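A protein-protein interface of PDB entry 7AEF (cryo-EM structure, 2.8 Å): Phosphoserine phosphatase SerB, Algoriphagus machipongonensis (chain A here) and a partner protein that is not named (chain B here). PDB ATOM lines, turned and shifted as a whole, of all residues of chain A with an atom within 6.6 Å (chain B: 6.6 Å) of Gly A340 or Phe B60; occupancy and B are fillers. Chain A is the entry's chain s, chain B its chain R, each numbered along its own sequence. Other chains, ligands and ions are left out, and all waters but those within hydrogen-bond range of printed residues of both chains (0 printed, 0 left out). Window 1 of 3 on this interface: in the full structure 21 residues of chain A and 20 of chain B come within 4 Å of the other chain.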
ATOM      1  N   VAL A  13       5.399  10.200  24.521  1.00  0.00           N
ATOM      2  CA  VAL A  13       6.101  10.645  23.325  1.00  0.00           C
ATOM      3  C   VAL A  13       5.478  10.111  22.036  1.00  0.00           C
ATOM      4  O   VAL A  13       6.076  10.191  20.969  1.00  0.00           O
ATOM      5  CB  VAL A  13       7.599  10.298  23.393  1.00  0.00           C
ATOM      6  CG1 VAL A  13       8.214  10.993  24.592  1.00  0.00           C
ATOM      7  CG2 VAL A  13       7.804   8.817  23.470  1.00  0.00           C
ATOM      8  N   ASP A  14       4.254   9.617  22.148  1.00  0.00           N
ATOM      9  CA  ASP A  14       3.445   9.119  21.040  1.00  0.00           C
ATOM     10  C   ASP A  14       3.131  10.141  19.943  1.00  0.00           C
ATOM     11  O   ASP A  14       3.000   9.768  18.781  1.00  0.00           O
ATOM     12  CB  ASP A  14       2.117   8.657  21.596  1.00  0.00           C
ATOM     13  CG  ASP A  14       2.229   7.440  22.375  1.00  0.00           C
ATOM     14  OD1 ASP A  14       3.119   6.668  22.142  1.00  0.00           O
ATOM     15  OD2 ASP A  14       1.495   7.327  23.330  1.00  0.00           O
ATOM     16  N   ARG A  15       2.955  11.421  20.287  1.00  0.00           N
ATOM     17  CA  ARG A  15       2.624  12.402  19.262  1.00  0.00           C
ATOM     18  C   ARG A  15       3.384  13.708  19.391  1.00  0.00           C
ATOM     19  O   ARG A  15       3.204  14.474  20.337  1.00  0.00           O
ATOM     20  CB  ARG A  15       1.131  12.675  19.301  1.00  0.00           C
ATOM     21  CG  ARG A  15       0.568  13.676  18.284  1.00  0.00           C
ATOM     22  CD  ARG A  15       0.651  13.188  16.917  1.00  0.00           C
ATOM     23  NE  ARG A  15      -0.245  13.899  16.031  1.00  0.00           N
ATOM     24  CZ  ARG A  15       0.023  15.001  15.299  1.00  0.00           C
ATOM     25  NH1 ARG A  15       1.185  15.612  15.311  1.00  0.00           N
ATOM     26  NH2 ARG A  15      -0.929  15.486  14.533  1.00  0.00           N
ATOM     27  N   VAL A  16       4.173  14.006  18.375  1.00  0.00           N
ATOM     28  CA  VAL A  16       4.968  15.221  18.329  1.00  0.00           C
ATOM     29  C   VAL A  16       4.198  16.297  17.593  1.00  0.00           C
ATOM     30  O   VAL A  16       3.665  16.038  16.511  1.00  0.00           O
ATOM     31  CB  VAL A  16       6.328  14.961  17.635  1.00  0.00           C
ATOM     32  CG1 VAL A  16       7.145  16.231  17.523  1.00  0.00           C
ATOM     33  CG2 VAL A  16       7.093  13.970  18.418  1.00  0.00           C
ATOM     34  N   ILE A 337      13.590  17.481  13.856  1.00  0.00           N
ATOM     35  CA  ILE A 337      12.211  17.026  13.958  1.00  0.00           C
ATOM     36  C   ILE A 337      11.666  16.576  12.613  1.00  0.00           C
ATOM     37  O   ILE A 337      11.527  17.366  11.674  1.00  0.00           O
ATOM     38  CB  ILE A 337      11.310  18.141  14.521  1.00  0.00           C
ATOM     39  CG1 ILE A 337      11.843  18.619  15.845  1.00  0.00           C
ATOM     40  CG2 ILE A 337       9.893  17.658  14.699  1.00  0.00           C
ATOM     41  CD1 ILE A 337      12.693  19.891  15.771  1.00  0.00           C
ATOM     42  N   SER A 338      11.371  15.285  12.503  1.00  0.00           N
ATOM     43  CA  SER A 338      10.853  14.732  11.250  1.00  0.00           C
ATOM     44  C   SER A 338      10.316  13.319  11.382  1.00  0.00           C
ATOM     45  O   SER A 338      10.729  12.554  12.254  1.00  0.00           O
ATOM     46  CB  SER A 338      11.914  14.727  10.161  1.00  0.00           C
ATOM     47  OG  SER A 338      12.955  13.841  10.458  1.00  0.00           O
ATOM     48  N   GLU A 339       9.409  12.961  10.478  1.00  0.00           N
ATOM     49  CA  GLU A 339       8.870  11.614  10.327  1.00  0.00           C
ATOM     50  C   GLU A 339       8.425  10.962  11.627  1.00  0.00           C
ATOM     51  O   GLU A 339       8.684   9.784  11.858  1.00  0.00           O
ATOM     52  CB  GLU A 339       9.868  10.719   9.598  1.00  0.00           C
ATOM     53  CG  GLU A 339      10.252  11.223   8.188  1.00  0.00           C
ATOM     54  CD  GLU A 339       9.105  11.199   7.147  1.00  0.00           C
ATOM     55  OE1 GLU A 339       8.163  10.480   7.331  1.00  0.00           O
ATOM     56  OE2 GLU A 339       9.199  11.930   6.172  1.00  0.00           O
ATOM     57  N   GLY A 340       7.723  11.713  12.468  1.00  0.00           N
ATOM     58  CA  GLY A 340       7.207  11.173  13.713  1.00  0.00           C
ATOM     59  C   GLY A 340       8.045  11.345  14.980  1.00  0.00           C
ATOM     60  O   GLY A 340       7.561  10.982  16.049  1.00  0.00           O
ATOM     61  N   ASN A 341       9.256  11.905  14.922  1.00  0.00           N
ATOM     62  CA  ASN A 341       9.988  12.048  16.180  1.00  0.00           C
ATOM     63  C   ASN A 341      10.887  13.279  16.267  1.00  0.00           C
ATOM     64  O   ASN A 341      11.281  13.887  15.273  1.00  0.00           O
ATOM     65  CB  ASN A 341      10.817  10.793  16.479  1.00  0.00           C
ATOM     66  CG  ASN A 341      11.160  10.640  17.995  1.00  0.00           C
ATOM     67  OD1 ASN A 341      10.620  11.407  18.815  1.00  0.00           O
ATOM     68  ND2 ASN A 341      12.003   9.716  18.367  1.00  0.00           N
ATOM     69  N   TRP A 342      11.174  13.642  17.507  1.00  0.00           N
ATOM     70  CA  TRP A 342      12.054  14.728  17.911  1.00  0.00           C
ATOM     71  C   TRP A 342      13.270  14.222  18.658  1.00  0.00           C
ATOM     72  O   TRP A 342      13.143  13.724  19.779  1.00  0.00           O
ATOM     73  CB  TRP A 342      11.280  15.702  18.803  1.00  0.00           C
ATOM     74  CG  TRP A 342      12.065  16.861  19.435  1.00  0.00           C
ATOM     75  CD1 TRP A 342      13.256  17.433  19.076  1.00  0.00           C
ATOM     76  CD2 TRP A 342      11.619  17.586  20.581  1.00  0.00           C
ATOM     77  NE1 TRP A 342      13.553  18.457  19.931  1.00  0.00           N
ATOM     78  CE2 TRP A 342      12.565  18.556  20.847  1.00  0.00           C
ATOM     79  CE3 TRP A 342      10.502  17.498  21.384  1.00  0.00           C
ATOM     80  CZ2 TRP A 342      12.417  19.431  21.887  1.00  0.00           C
ATOM     81  CZ3 TRP A 342      10.366  18.372  22.420  1.00  0.00           C
ATOM     82  CH2 TRP A 342      11.294  19.312  22.661  1.00  0.00           C
ATOM     83  N   VAL B  43      -1.264   2.607   7.467  1.00  0.00           N
ATOM     84  CA  VAL B  43      -0.884   3.600   8.471  1.00  0.00           C
ATOM     85  C   VAL B  43       0.573   3.364   8.838  1.00  0.00           C
ATOM     86  O   VAL B  43       0.977   2.222   9.083  1.00  0.00           O
ATOM     87  CB  VAL B  43      -1.776   3.540   9.735  1.00  0.00           C
ATOM     88  CG1 VAL B  43      -1.455   4.690  10.671  1.00  0.00           C
ATOM     89  CG2 VAL B  43      -3.239   3.592   9.382  1.00  0.00           C
ATOM     90  N   GLU B  44       1.364   4.437   8.853  1.00  0.00           N
ATOM     91  CA  GLU B  44       2.799   4.360   9.113  1.00  0.00           C
ATOM     92  C   GLU B  44       3.205   4.920  10.473  1.00  0.00           C
ATOM     93  O   GLU B  44       2.724   5.970  10.902  1.00  0.00           O
ATOM     94  CB  GLU B  44       3.579   5.067   8.002  1.00  0.00           C
ATOM     95  CG  GLU B  44       5.086   5.063   8.197  1.00  0.00           C
ATOM     96  CD  GLU B  44       5.822   5.772   7.084  1.00  0.00           C
ATOM     97  OE1 GLU B  44       5.153   6.337   6.195  1.00  0.00           O
ATOM     98  OE2 GLU B  44       7.070   5.803   7.118  1.00  0.00           O
ATOM     99  N   GLN B  45       4.105   4.205  11.145  1.00  0.00           N
ATOM    100  CA  GLN B  45       4.582   4.591  12.464  1.00  0.00           C
ATOM    101  C   GLN B  45       6.099   4.705  12.478  1.00  0.00           C
ATOM    102  O   GLN B  45       6.789   4.168  11.614  1.00  0.00           O
ATOM    103  CB  GLN B  45       4.154   3.588  13.542  1.00  0.00           C
ATOM    104  CG  GLN B  45       2.710   3.688  13.953  1.00  0.00           C
ATOM    105  CD  GLN B  45       1.861   2.659  13.267  1.00  0.00           C
ATOM    106  OE1 GLN B  45       2.372   1.719  12.682  1.00  0.00           O
ATOM    107  NE2 GLN B  45       0.555   2.838  13.324  1.00  0.00           N
ATOM    108  N   ASN B  46       6.608   5.424  13.475  1.00  0.00           N
ATOM    109  CA  ASN B  46       8.042   5.580  13.705  1.00  0.00           C
ATOM    110  C   ASN B  46       8.457   4.646  14.835  1.00  0.00           C
ATOM    111  O   ASN B  46       7.887   4.707  15.928  1.00  0.00           O
ATOM    112  CB  ASN B  46       8.363   7.034  14.048  1.00  0.00           C
ATOM    113  CG  ASN B  46       9.848   7.318  14.086  1.00  0.00           C
ATOM    114  OD1 ASN B  46      10.494   7.155  15.109  1.00  0.00           O
ATOM    115  ND2 ASN B  46      10.387   7.768  12.972  1.00  0.00           N
ATOM    116  N   ILE B  58       5.742   2.902  20.048  1.00  0.00           N
ATOM    117  CA  ILE B  58       5.604   3.265  18.649  1.00  0.00           C
ATOM    118  C   ILE B  58       4.808   4.536  18.459  1.00  0.00           C
ATOM    119  O   ILE B  58       3.781   4.704  19.039  1.00  0.00           O
ATOM    120  CB  ILE B  58       5.063   2.081  17.840  1.00  0.00           C
ATOM    121  CG1 ILE B  58       3.713   1.612  18.375  1.00  0.00           C
ATOM    122  CG2 ILE B  58       6.063   0.949  17.900  1.00  0.00           C
ATOM    123  CD1 ILE B  58       3.036   0.586  17.507  1.00  0.00           C
ATOM    124  N   ARG B  59       5.288   5.406  17.584  1.00  0.00           N
ATOM    125  CA  ARG B  59       4.713   6.720  17.363  1.00  0.00           C
ATOM    126  C   ARG B  59       3.981   6.871  16.063  1.00  0.00           C
ATOM    127  O   ARG B  59       4.364   6.273  15.111  1.00  0.00           O
ATOM    128  CB  ARG B  59       5.842   7.739  17.371  1.00  0.00           C
ATOM    129  CG  ARG B  59       6.879   7.574  18.452  1.00  0.00           C
ATOM    130  CD  ARG B  59       8.140   8.321  18.112  1.00  0.00           C
ATOM    131  NE  ARG B  59       9.138   8.232  19.162  1.00  0.00           N
ATOM    132  CZ  ARG B  59       9.981   7.224  19.344  1.00  0.00           C
ATOM    133  NH1 ARG B  59       9.975   6.187  18.549  1.00  0.00           N
ATOM    134  NH2 ARG B  59      10.841   7.263  20.327  1.00  0.00           N
ATOM    135  N   PHE B  60       2.920   7.661  16.025  1.00  0.00           N
ATOM    136  CA  PHE B  60       2.172   7.931  14.797  1.00  0.00           C
ATOM    137  C   PHE B  60       2.977   8.794  13.843  1.00  0.00           C
ATOM    138  O   PHE B  60       3.536   9.776  14.234  1.00  0.00           O
ATOM    139  CB  PHE B  60       0.854   8.638  15.146  1.00  0.00           C
ATOM    140  CG  PHE B  60       0.070   9.145  13.963  1.00  0.00           C
ATOM    141  CD1 PHE B  60      -0.426   8.282  13.023  1.00  0.00           C
ATOM    142  CD2 PHE B  60      -0.187  10.488  13.811  1.00  0.00           C
ATOM    143  CE1 PHE B  60      -1.148   8.750  11.959  1.00  0.00           C
ATOM    144  CE2 PHE B  60      -0.888  10.963  12.732  1.00  0.00           C
ATOM    145  CZ  PHE B  60      -1.371  10.090  11.801  1.00  0.00           C
ATOM    146  N   ASN B  61       3.023   8.407  12.582  1.00  0.00           N
ATOM    147  CA  ASN B  61       3.680   9.172  11.550  1.00  0.00           C
ATOM    148  C   ASN B  61       2.584   9.766  10.642  1.00  0.00           C
ATOM    149  O   ASN B  61       2.227  10.901  10.804  1.00  0.00           O
ATOM    150  CB  ASN B  61       4.701   8.305  10.792  1.00  0.00           C
ATOM    151  CG  ASN B  61       5.506   9.063   9.757  1.00  0.00           C
ATOM    152  OD1 ASN B  61       5.304  10.207   9.510  1.00  0.00           O
ATOM    153  ND2 ASN B  61       6.410   8.393   9.144  1.00  0.00           N
ATOM    154  N   LYS B  62       1.991   8.985   9.753  1.00  0.00           N
ATOM    155  CA  LYS B  62       0.978   9.488   8.827  1.00  0.00           C
ATOM    156  C   LYS B  62       0.103   8.427   8.214  1.00  0.00           C
ATOM    157  O   LYS B  62       0.384   7.282   8.324  1.00  0.00           O
ATOM    158  CB  LYS B  62       1.601  10.317   7.716  1.00  0.00           C
ATOM    159  CG  LYS B  62       2.371   9.550   6.696  1.00  0.00           C
ATOM    160  CD  LYS B  62       3.394  10.468   6.136  1.00  0.00           C
ATOM    161  CE  LYS B  62       4.495   9.692   5.483  1.00  0.00           C
ATOM    162  NZ  LYS B  62       5.629  10.604   5.280  1.00  0.00           N
ATOM    163  N   ILE B  63      -0.980   8.833   7.582  1.00  0.00           N
ATOM    164  CA  ILE B  63      -1.880   7.914   6.929  1.00  0.00           C
ATOM    165  C   ILE B  63      -1.678   8.040   5.422  1.00  0.00           C
ATOM    166  O   ILE B  63      -1.800   9.109   4.871  1.00  0.00           O
ATOM    167  CB  ILE B  63      -3.332   8.190   7.344  1.00  0.00           C
ATOM    168  CG1 ILE B  63      -3.485   8.016   8.839  1.00  0.00           C
ATOM    169  CG2 ILE B  63      -4.291   7.241   6.688  1.00  0.00           C
ATOM    170  CD1 ILE B  63      -4.743   8.576   9.413  1.00  0.00           C
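The side-chain amino group (NZ) of Lys B62 is in salt-bridge range of the side-chain carboxylate (OE1) of Glu A339.
ND2 of Asn B61 sits at hydrogen-bond distance from OE1 of Glu A339 (3.3 Å).
The guanidinium group (NE) of Arg B59 sits close to the side-chain amide nitrogen (ND2) of Asn A341 (3.3 Å).
The side-chain amide nitrogen (ND2) of Asn B46 lies within hydrogen-bond range of the backbone carbonyl oxygen (O) of Glu A339 (2.9 Å).
The backbone NH (N) of Phe B60 is in hydrogen-bond range of the backbone carbonyl oxygen (O) of Asp A14 (3.5 Å).
The backbone NH of Glu B44 lies within hydrogen-bond range of the backbone carbonyl oxygen of Lys B62 (3.1 Å).
N of Asn B46 lies within hydrogen-bond range of O of Arg B59 (2.9 Å).
The backbone carbonyl oxygen of Glu B44 sits at hydrogen-bond distance from the backbone NH of Asn B61.
Among the printed residues, merely in contact across the chains: Gly A340 with Arg B59 (3.4 Å), Val A13 with Arg B59 (3.7 Å), Asp A14 with Ile B58 (3.7 Å), Asp A14 with Arg B59 (3.8 Å), Asn A341 with Asn B46 (3.9 Å) and Gly A340 with Phe B60 (3.96 Å).
Of the printed residues of chain B, Asp A14 touches Ile B58, Arg B59 and Phe B60.
Ile A337 touches none of the printed residues of chain B.
Of chain B, only Arg B59 and Phe B60 come within 4 Å of Gly A340.
Printed residues of chain B within 4 Å of Asn A341: Asn B46 (3.9 Å) and Arg B59 (3.3 Å).
Of the printed residues of chain A, Arg B59 touches Val A13, Asp A14, Gly A340 and Asn A341.
Printed residues of chain A within 4 Å of Asn B61: Glu A339.
The nearest residue of chain B that does not touch Gly A340 is Asn B61 (4.1 Å).
Of the 10 printed residues of chain A, 5 touch a printed residue of chain B.
Along chain A the printed residues that touch a printed residue of chain B span positions 13 to 341.
Among the printed residues, Asp or Glu carboxylates within 4 Å of a Lys or Arg side-chain nitrogen of the other chain: Glu A339 with Lys B62 (3.3 Å).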
